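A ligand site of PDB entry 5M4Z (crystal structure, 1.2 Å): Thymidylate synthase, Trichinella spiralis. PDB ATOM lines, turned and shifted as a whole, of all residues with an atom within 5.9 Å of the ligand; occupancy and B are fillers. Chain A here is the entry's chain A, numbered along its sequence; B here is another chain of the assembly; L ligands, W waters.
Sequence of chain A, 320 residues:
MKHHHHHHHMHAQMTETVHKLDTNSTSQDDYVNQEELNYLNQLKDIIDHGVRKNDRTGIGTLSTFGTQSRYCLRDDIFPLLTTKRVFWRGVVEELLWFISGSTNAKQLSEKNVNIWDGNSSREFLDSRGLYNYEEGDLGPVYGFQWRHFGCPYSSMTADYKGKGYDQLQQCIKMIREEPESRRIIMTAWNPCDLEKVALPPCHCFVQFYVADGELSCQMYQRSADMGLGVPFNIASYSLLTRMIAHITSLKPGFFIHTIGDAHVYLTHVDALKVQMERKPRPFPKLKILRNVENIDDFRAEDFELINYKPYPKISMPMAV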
ATOM      1  N   GLU A  94       6.344   2.284   8.401  1.00  0.00           N
ATOM      2  CA  GLU A  94       7.045   3.546   8.210  1.00  0.00           C
ATOM      3  C   GLU A  94       7.719   3.606   6.851  1.00  0.00           C
ATOM      4  O   GLU A  94       7.714   4.660   6.187  1.00  0.00           O
ATOM      5  CB  GLU A  94       8.074   3.773   9.328  1.00  0.00           C
ATOM      6  CG  GLU A  94       8.721   5.150   9.252  1.00  0.00           C
ATOM      7  CD  GLU A  94      10.078   5.237   9.881  1.00  0.00           C
ATOM      8  OE1 GLU A  94      10.915   4.333   9.675  1.00  0.00           O
ATOM      9  OE2 GLU A  94      10.316   6.249  10.561  1.00  0.00           O
ATOM     10  N   PHE A  98       7.226   6.353   3.978  1.00  0.00           N
ATOM     11  CA  PHE A  98       8.314   7.122   3.348  1.00  0.00           C
ATOM     12  C   PHE A  98       8.250   7.021   1.824  1.00  0.00           C
ATOM     13  O   PHE A  98       8.370   8.026   1.103  1.00  0.00           O
ATOM     14  CB  PHE A  98       9.706   6.564   3.716  1.00  0.00           C
ATOM     15  CG  PHE A  98      10.209   6.835   5.122  1.00  0.00           C
ATOM     16  CD1 PHE A  98       9.746   7.889   5.920  1.00  0.00           C
ATOM     17  CD2 PHE A  98      11.208   5.986   5.625  1.00  0.00           C
ATOM     18  CE1 PHE A  98      10.273   8.100   7.166  1.00  0.00           C
ATOM     19  CE2 PHE A  98      11.730   6.178   6.893  1.00  0.00           C
ATOM     20  CZ  PHE A  98      11.294   7.235   7.656  1.00  0.00           C
ATOM     21  N   TRP A 116       6.012   8.714  15.128  1.00  0.00           N
ATOM     22  CA  TRP A 116       6.258  10.098  14.756  1.00  0.00           C
ATOM     23  C   TRP A 116       5.281  11.061  15.428  1.00  0.00           C
ATOM     24  O   TRP A 116       5.330  12.262  15.156  1.00  0.00           O
ATOM     25  CB  TRP A 116       6.237  10.267  13.219  1.00  0.00           C
ATOM     26  CG  TRP A 116       7.461   9.760  12.579  1.00  0.00           C
ATOM     27  CD1 TRP A 116       7.631   8.616  11.884  1.00  0.00           C
ATOM     28  CD2 TRP A 116       8.728  10.398  12.589  1.00  0.00           C
ATOM     29  NE1 TRP A 116       8.924   8.477  11.459  1.00  0.00           N
ATOM     30  CE2 TRP A 116       9.623   9.570  11.885  1.00  0.00           C
ATOM     31  CE3 TRP A 116       9.196  11.582  13.158  1.00  0.00           C
ATOM     32  CZ2 TRP A 116      10.955   9.895  11.717  1.00  0.00           C
ATOM     33  CZ3 TRP A 116      10.524  11.915  12.988  1.00  0.00           C
ATOM     34  CH2 TRP A 116      11.396  11.076  12.275  1.00  0.00           C
ATOM     35  N   TYR A 142      11.876  12.849   5.283  1.00  0.00           N
ATOM     36  CA  TYR A 142      12.326  11.772   4.406  1.00  0.00           C
ATOM     37  C   TYR A 142      11.494  11.606   3.144  1.00  0.00           C
ATOM     38  O   TYR A 142      12.024  11.695   2.032  1.00  0.00           O
ATOM     39  CB  TYR A 142      12.369  10.450   5.188  1.00  0.00           C
ATOM     40  CG  TYR A 142      13.242  10.479   6.407  1.00  0.00           C
ATOM     41  CD1 TYR A 142      14.615  10.315   6.307  1.00  0.00           C
ATOM     42  CD2 TYR A 142      12.710  10.699   7.660  1.00  0.00           C
ATOM     43  CE1 TYR A 142      15.404  10.338   7.414  1.00  0.00           C
ATOM     44  CE2 TYR A 142      13.494  10.723   8.780  1.00  0.00           C
ATOM     45  CZ  TYR A 142      14.851  10.537   8.661  1.00  0.00           C
ATOM     46  OH  TYR A 142      15.685  10.535   9.771  1.00  0.00           O
ATOM     47  N   LEU A 199      12.024  17.824  12.659  1.00  0.00           N
ATOM     48  CA  LEU A 199      13.264  17.195  13.098  1.00  0.00           C
ATOM     49  C   LEU A 199      14.089  17.028  11.826  1.00  0.00           C
ATOM     50  O   LEU A 199      13.586  16.479  10.849  1.00  0.00           O
ATOM     51  CB  LEU A 199      12.983  15.825  13.735  1.00  0.00           C
ATOM     52  CG  LEU A 199      14.155  15.019  14.299  1.00  0.00           C
ATOM     53  CD1 LEU A 199      14.778  15.764  15.470  1.00  0.00           C
ATOM     54  CD2 LEU A 199      13.742  13.609  14.718  1.00  0.00           C
ATOM     55  N   PRO A 200      15.338  17.436  11.787  1.00  0.00           N
ATOM     56  CA  PRO A 200      16.168  17.182  10.608  1.00  0.00           C
ATOM     57  C   PRO A 200      16.415  15.696  10.451  1.00  0.00           C
ATOM     58  O   PRO A 200      16.637  14.999  11.445  1.00  0.00           O
ATOM     59  CB  PRO A 200      17.460  17.946  10.927  1.00  0.00           C
ATOM     60  CG  PRO A 200      16.984  19.029  11.824  1.00  0.00           C
ATOM     61  CD  PRO A 200      16.009  18.336  12.723  1.00  0.00           C
ATOM     62  N   CYS A 202      17.835  12.117  10.376  1.00  0.00           N
ATOM     63  CA  CYS A 202      18.952  11.438  11.015  1.00  0.00           C
ATOM     64  C   CYS A 202      19.661  10.523  10.031  1.00  0.00           C
ATOM     65  O   CYS A 202      20.890  10.465   9.984  1.00  0.00           O
ATOM     66  CB  CYS A 202      18.453  10.579  12.198  1.00  0.00           C
ATOM     67  SG  CYS A 202      17.847  11.397  13.725  1.00  0.00           S
ATOM     68  N   HIS A 203      18.913   9.751   9.261  1.00  0.00           N
ATOM     69  CA  HIS A 203      19.450   8.884   8.226  1.00  0.00           C
ATOM     70  C   HIS A 203      19.451   9.720   6.940  1.00  0.00           C
ATOM     71  O   HIS A 203      18.423   9.891   6.297  1.00  0.00           O
ATOM     72  CB  HIS A 203      18.770   7.496   8.170  1.00  0.00           C
ATOM     73  CG  HIS A 203      17.297   7.440   8.461  1.00  0.00           C
ATOM     74  ND1 HIS A 203      16.378   7.338   7.442  1.00  0.00           N
ATOM     75  CD2 HIS A 203      16.585   7.347   9.606  1.00  0.00           C
ATOM     76  CE1 HIS A 203      15.158   7.215   7.944  1.00  0.00           C
ATOM     77  NE2 HIS A 203      15.257   7.250   9.259  1.00  0.00           N
ATOM     78  N   GLN A 221      24.250   7.913   8.738  1.00  0.00           N
ATOM     79  CA  GLN A 221      23.358   8.398   9.780  1.00  0.00           C
ATOM     80  C   GLN A 221      24.126   9.400  10.645  1.00  0.00           C
ATOM     81  O   GLN A 221      25.075   9.023  11.313  1.00  0.00           O
ATOM     82  CB  GLN A 221      22.870   7.201  10.586  1.00  0.00           C
ATOM     83  CG  GLN A 221      21.927   7.560  11.701  1.00  0.00           C
ATOM     84  CD  GLN A 221      21.066   6.393  12.166  1.00  0.00           C
ATOM     85  OE1 GLN A 221      21.174   5.275  11.696  1.00  0.00           O
ATOM     86  NE2 GLN A 221      20.216   6.666  13.126  1.00  0.00           N
ATOM     87  N   ARG A 222      23.699  10.660  10.634  1.00  0.00           N
ATOM     88  CA  ARG A 222      24.434  11.683  11.364  1.00  0.00           C
ATOM     89  C   ARG A 222      24.374  11.509  12.879  1.00  0.00           C
ATOM     90  O   ARG A 222      25.255  11.981  13.600  1.00  0.00           O
ATOM     91  CB  ARG A 222      23.908  13.071  10.982  1.00  0.00           C
ATOM     92  CG  ARG A 222      22.482  13.318  11.396  1.00  0.00           C
ATOM     93  CD  ARG A 222      22.020  14.774  11.146  1.00  0.00           C
ATOM     94  NE  ARG A 222      20.656  14.936  11.603  1.00  0.00           N
ATOM     95  CZ  ARG A 222      20.276  15.057  12.867  1.00  0.00           C
ATOM     96  NH1 ARG A 222      21.188  15.134  13.841  1.00  0.00           N
ATOM     97  NH2 ARG A 222      18.993  15.069  13.154  1.00  0.00           N
ATOM     98  N   SER A 223      23.321  10.864  13.362  1.00  0.00           N
ATOM     99  CA  SER A 223      23.012  10.781  14.772  1.00  0.00           C
ATOM    100  C   SER A 223      22.237   9.505  14.989  1.00  0.00           C
ATOM    101  O   SER A 223      21.215   9.297  14.325  1.00  0.00           O
ATOM    102  CB  SER A 223      22.181  11.989  15.176  1.00  0.00           C
ATOM    103  OG  SER A 223      21.866  11.928  16.545  1.00  0.00           O
ATOM    104  N   ALA A 224      22.711   8.659  15.891  1.00  0.00           N
ATOM    105  CA  ALA A 224      22.124   7.334  16.082  1.00  0.00           C
ATOM    106  C   ALA A 224      22.044   7.042  17.561  1.00  0.00           C
ATOM    107  O   ALA A 224      23.060   6.998  18.250  1.00  0.00           O
ATOM    108  CB  ALA A 224      22.965   6.276  15.391  1.00  0.00           C
ATOM    109  N   ASP A 225      20.835   6.759  18.020  1.00  0.00           N
ATOM    110  CA  ASP A 225      20.612   6.240  19.352  1.00  0.00           C
ATOM    111  C   ASP A 225      20.820   4.750  19.248  1.00  0.00           C
ATOM    112  O   ASP A 225      20.010   4.025  18.649  1.00  0.00           O
ATOM    113  CB  ASP A 225      19.191   6.562  19.791  1.00  0.00           C
ATOM    114  CG  ASP A 225      18.859   6.031  21.175  1.00  0.00           C
ATOM    115  OD1 ASP A 225      19.629   5.184  21.671  1.00  0.00           O
ATOM    116  OD2 ASP A 225      17.852   6.475  21.771  1.00  0.00           O
ATOM    117  N   MET A 226      21.931   4.275  19.772  1.00  0.00           N
ATOM    118  CA  MET A 226      22.320   2.892  19.605  1.00  0.00           C
ATOM    119  C   MET A 226      21.332   1.941  20.233  1.00  0.00           C
ATOM    120  O   MET A 226      21.193   0.800  19.773  1.00  0.00           O
ATOM    121  CB  MET A 226      23.716   2.659  20.175  1.00  0.00           C
ATOM    122  CG  MET A 226      24.827   3.227  19.350  1.00  0.00           C
ATOM    123  SD  MET A 226      25.130   2.267  17.860  1.00  0.00           S
ATOM    124  CE  MET A 226      25.788   0.749  18.541  1.00  0.00           C
ATOM    125  N   LEU A 228      17.787   2.371  20.942  1.00  0.00           N
ATOM    126  CA  LEU A 228      16.419   2.321  20.442  1.00  0.00           C
ATOM    127  C   LEU A 228      16.323   2.533  18.942  1.00  0.00           C
ATOM    128  O   LEU A 228      15.539   1.869  18.271  1.00  0.00           O
ATOM    129  CB  LEU A 228      15.556   3.375  21.155  1.00  0.00           C
ATOM    130  CG  LEU A 228      15.272   3.085  22.629  1.00  0.00           C
ATOM    131  CD1 LEU A 228      14.570   4.270  23.278  1.00  0.00           C
ATOM    132  CD2 LEU A 228      14.435   1.823  22.785  1.00  0.00           C
ATOM    133  N   GLY A 229      17.123   3.420  18.387  1.00  0.00           N
ATOM    134  CA  GLY A 229      17.011   3.761  16.992  1.00  0.00           C
ATOM    135  C   GLY A 229      17.718   2.784  16.080  1.00  0.00           C
ATOM    136  O   GLY A 229      17.122   2.319  15.108  1.00  0.00           O
ATOM    137  N   VAL A 230      18.981   2.487  16.373  1.00  0.00           N
ATOM    138  CA  VAL A 230      19.814   1.744  15.428  1.00  0.00           C
ATOM    139  C   VAL A 230      19.204   0.421  15.000  1.00  0.00           C
ATOM    140  O   VAL A 230      19.201   0.141  13.791  1.00  0.00           O
ATOM    141  CB  VAL A 230      21.252   1.614  15.983  1.00  0.00           C
ATOM    142  CG1 VAL A 230      22.050   0.531  15.263  1.00  0.00           C
ATOM    143  CG2 VAL A 230      21.974   2.948  15.870  1.00  0.00           C
ATOM    144  N   ASN A 233      16.569   1.203  12.490  1.00  0.00           N
ATOM    145  CA  ASN A 233      17.134   1.783  11.277  1.00  0.00           C
ATOM    146  C   ASN A 233      17.847   0.739  10.403  1.00  0.00           C
ATOM    147  O   ASN A 233      17.758   0.795   9.174  1.00  0.00           O
ATOM    148  CB  ASN A 233      18.151   2.879  11.659  1.00  0.00           C
ATOM    149  CG  ASN A 233      17.571   4.002  12.538  1.00  0.00           C
ATOM    150  OD1 ASN A 233      18.280   4.524  13.404  1.00  0.00           O
ATOM    151  ND2 ASN A 233      16.332   4.399  12.299  1.00  0.00           N
ATOM    152  N   HIS A 263      25.488   7.100  19.916  1.00  0.00           N
ATOM    153  CA  HIS A 263      25.369   7.422  21.333  1.00  0.00           C
ATOM    154  C   HIS A 263      24.357   6.547  22.044  1.00  0.00           C
ATOM    155  O   HIS A 263      23.495   5.911  21.442  1.00  0.00           O
ATOM    156  CB  HIS A 263      25.054   8.920  21.525  1.00  0.00           C
ATOM    157  CG  HIS A 263      23.836   9.368  20.792  1.00  0.00           C
ATOM    158  ND1 HIS A 263      23.888   9.907  19.525  1.00  0.00           N
ATOM    159  CD2 HIS A 263      22.521   9.295  21.105  1.00  0.00           C
ATOM    160  CE1 HIS A 263      22.661  10.168  19.104  1.00  0.00           C
ATOM    161  NE2 HIS A 263      21.812   9.805  20.046  1.00  0.00           N
ATOM    162  N   TYR A 265      21.924   7.018  25.703  1.00  0.00           N
ATOM    163  CA  TYR A 265      21.505   7.930  26.763  1.00  0.00           C
ATOM    164  C   TYR A 265      21.901   7.369  28.126  1.00  0.00           C
ATOM    165  O   TYR A 265      21.771   6.162  28.376  1.00  0.00           O
ATOM    166  CB  TYR A 265      20.002   8.179  26.651  1.00  0.00           C
ATOM    167  CG  TYR A 265      19.725   9.064  25.463  1.00  0.00           C
ATOM    168  CD1 TYR A 265      19.804  10.438  25.596  1.00  0.00           C
ATOM    169  CD2 TYR A 265      19.450   8.535  24.205  1.00  0.00           C
ATOM    170  CE1 TYR A 265      19.577  11.268  24.514  1.00  0.00           C
ATOM    171  CE2 TYR A 265      19.227   9.357  23.125  1.00  0.00           C
ATOM    172  CZ  TYR A 265      19.304  10.727  23.296  1.00  0.00           C
ATOM    173  OH  TYR A 265      19.083  11.569  22.253  1.00  0.00           O
ATOM    174  N   ARG B 182      24.508  17.519  16.836  1.00  0.00           N
ATOM    175  CA  ARG B 182      24.654  16.357  15.961  1.00  0.00           C
ATOM    176  C   ARG B 182      24.240  16.663  14.536  1.00  0.00           C
ATOM    177  O   ARG B 182      24.048  15.728  13.724  1.00  0.00           O
ATOM    178  CB  ARG B 182      23.876  15.188  16.554  1.00  0.00           C
ATOM    179  CG  ARG B 182      24.392  14.821  17.961  1.00  0.00           C
ATOM    180  CD  ARG B 182      23.738  13.600  18.580  1.00  0.00           C
ATOM    181  NE  ARG B 182      22.353  13.897  18.945  1.00  0.00           N
ATOM    182  CZ  ARG B 182      21.841  13.797  20.170  1.00  0.00           C
ATOM    183  NH1 ARG B 182      22.544  13.321  21.193  1.00  0.00           N
ATOM    184  NH2 ARG B 182      20.580  14.120  20.366  1.00  0.00           N
ATOM    185  N   ARG B 183      24.118  17.946  14.211  1.00  0.00           N
ATOM    186  CA  ARG B 183      23.614  18.437  12.934  1.00  0.00           C
ATOM    187  C   ARG B 183      24.636  19.347  12.216  1.00  0.00           C
ATOM    188  O   ARG B 183      24.226  20.160  11.393  1.00  0.00           O
ATOM    189  CB  ARG B 183      22.262  19.180  13.147  1.00  0.00           C
ATOM    190  CG  ARG B 183      21.225  18.394  13.948  1.00  0.00           C
ATOM    191  CD  ARG B 183      20.060  19.270  14.445  1.00  0.00           C
ATOM    192  NE  ARG B 183      19.038  18.464  15.132  1.00  0.00           N
ATOM    193  CZ  ARG B 183      17.893  18.950  15.584  1.00  0.00           C
ATOM    194  NH1 ARG B 183      17.583  20.220  15.403  1.00  0.00           N
ATOM    195  NH2 ARG B 183      17.039  18.140  16.189  1.00  0.00           N
HETATM  196  O1  LIG L   1      18.536   7.104  16.034  1.00  0.00           O
HETATM  197  C1  LIG L   1      17.810   7.862  15.358  1.00  0.00           C
HETATM  198  N1  LIG L   1      17.175   7.378  14.282  1.00  0.00           N
HETATM  199  C2  LIG L   1      16.186   8.066  13.689  1.00  0.00           C
HETATM  200  N2  LIG L   1      15.426   7.491  12.832  1.00  0.00           N
HETATM  201  O2  LIG L   1      14.355   8.191  12.246  1.00  0.00           O
HETATM  202  C3  LIG L   1      15.902   9.507  14.101  1.00  0.00           C
HETATM  203  C4  LIG L   1      17.095  10.182  14.790  1.00  0.00           C
HETATM  204  N3  LIG L   1      17.598   9.140  15.702  1.00  0.00           N
HETATM  205  C5  LIG L   1      17.910   9.575  17.064  1.00  0.00           C
HETATM  206  C6  LIG L   1      19.339  10.129  17.132  1.00  0.00           C
HETATM  207  C7  LIG L   1      19.218  11.088  18.289  1.00  0.00           C
HETATM  208  O3  LIG L   1      19.266  10.414  19.558  1.00  0.00           O
HETATM  209  O4  LIG L   1      17.065  10.644  17.519  1.00  0.00           O
HETATM  210  C8  LIG L   1      17.837  11.704  18.102  1.00  0.00           C
HETATM  211  C9  LIG L   1      17.814  12.884  17.150  1.00  0.00           C
HETATM  212  O5  LIG L   1      18.329  14.044  17.813  1.00  0.00           O
HETATM  213  P1  LIG L   1      19.341  15.034  17.077  1.00  0.00           P
HETATM  214  O6  LIG L   1      18.613  15.676  15.903  1.00  0.00           O
HETATM  215  O7  LIG L   1      19.684  16.052  18.163  1.00  0.00           O
HETATM  216  O8  LIG L   1      20.553  14.237  16.644  1.00  0.00           O
HETATM  217  O   HOH W   1      13.073   6.324  10.643  1.00  0.00           O
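Merely in contact with the ligand: Trp 116, Tyr 142, Leu 199, Ala 224 and Gly 229. Hydrophobic or aromatic side chains within 4 Å of the ligand: Trp 116, Leu 199, His 203, His 263 and Tyr 265. Within 4 Å of the ligand: Trp 116, Tyr 142, Leu 199, Cys 202, His 203, Gln 221, Arg 222, Ser 223, Ala 224, Asp 225, Gly 229, Asn 233, His 263, Tyr 265, Arg 182 of chain B and Arg 183 of chain B. The nearest printed residue that does not touch the ligand is Val 230 (4.7 Å).
Water W1 lies within hydrogen-bond range of a ring nitrogen (NE2) of His 203 (2.7 Å), the side-chain carboxylate (OE2) of Glu 94 (2.8 Å) and an oxygen (O2) of the ligand (2.8 Å).
O of Cys 202 sits at hydrogen-bond distance from N of Arg 222. The backbone NH of Cys 202 is in hydrogen-bond range of the side-chain hydroxyl of Tyr 142 (2.7 Å). O of Ala 224 sits at hydrogen-bond distance from N of His 263, 2.9 Å away. The backbone carbonyl oxygen (O) of Arg 182 of chain B sits at hydrogen-bond distance from the guanidinium group (NH1) of Arg 222 (2.9 Å). OD1 of Asp 225 sits at hydrogen-bond distance from N of Leu 228. The side-chain amide nitrogen (NE2) of Gln 221 sits at hydrogen-bond distance from the side-chain amide oxygen (OD1) of Asn 233, 2.9 Å away. A ring nitrogen (NE2) of His 203 lies close to the side-chain hydroxyl of Tyr 142. The indole nitrogen (NE1) of Trp 116 is in hydrogen-bond range of the side-chain carboxylate (OE2) of Glu 94 (2.8 Å).
The side-chain sulfur (SG) of Cys 202 is bonded to a carbon (C4) of the ligand, 1.8 Å away. An oxygen (O8) of the ligand sits at hydrogen-bond distance from the side-chain hydroxyl (OG) of Ser 223, 2.7 Å away. An oxygen (O3) of the ligand sits at hydrogen-bond distance from a ring nitrogen (NE2) of His 263 (2.7 Å). NH2 of Arg 222 is in salt-bridge range of O6 of the ligand (2.8 Å). NE of Arg 183 of chain B is in salt-bridge range of O6 of the ligand (2.9 Å). The side-chain hydroxyl (OH) of Tyr 265 lies within hydrogen-bond range of an oxygen (O3) of the ligand, 2.9 Å away. O8 of the ligand lies within salt-bridge range of NE of Arg 182 of chain B. The backbone NH (N) of Asp 225 is in hydrogen-bond range of an oxygen (O1) of the ligand, 3.1 Å away. The side-chain amide oxygen of Asn 233 is in hydrogen-bond range of a nitrogen (N1) of the ligand. NE2 of His 203 is in hydrogen-bond range of O2 of the ligand (3.3 Å). The side-chain amide nitrogen (NE2) of Gln 221 sits close to a nitrogen (N1) of the ligand, 3.3 Å away.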
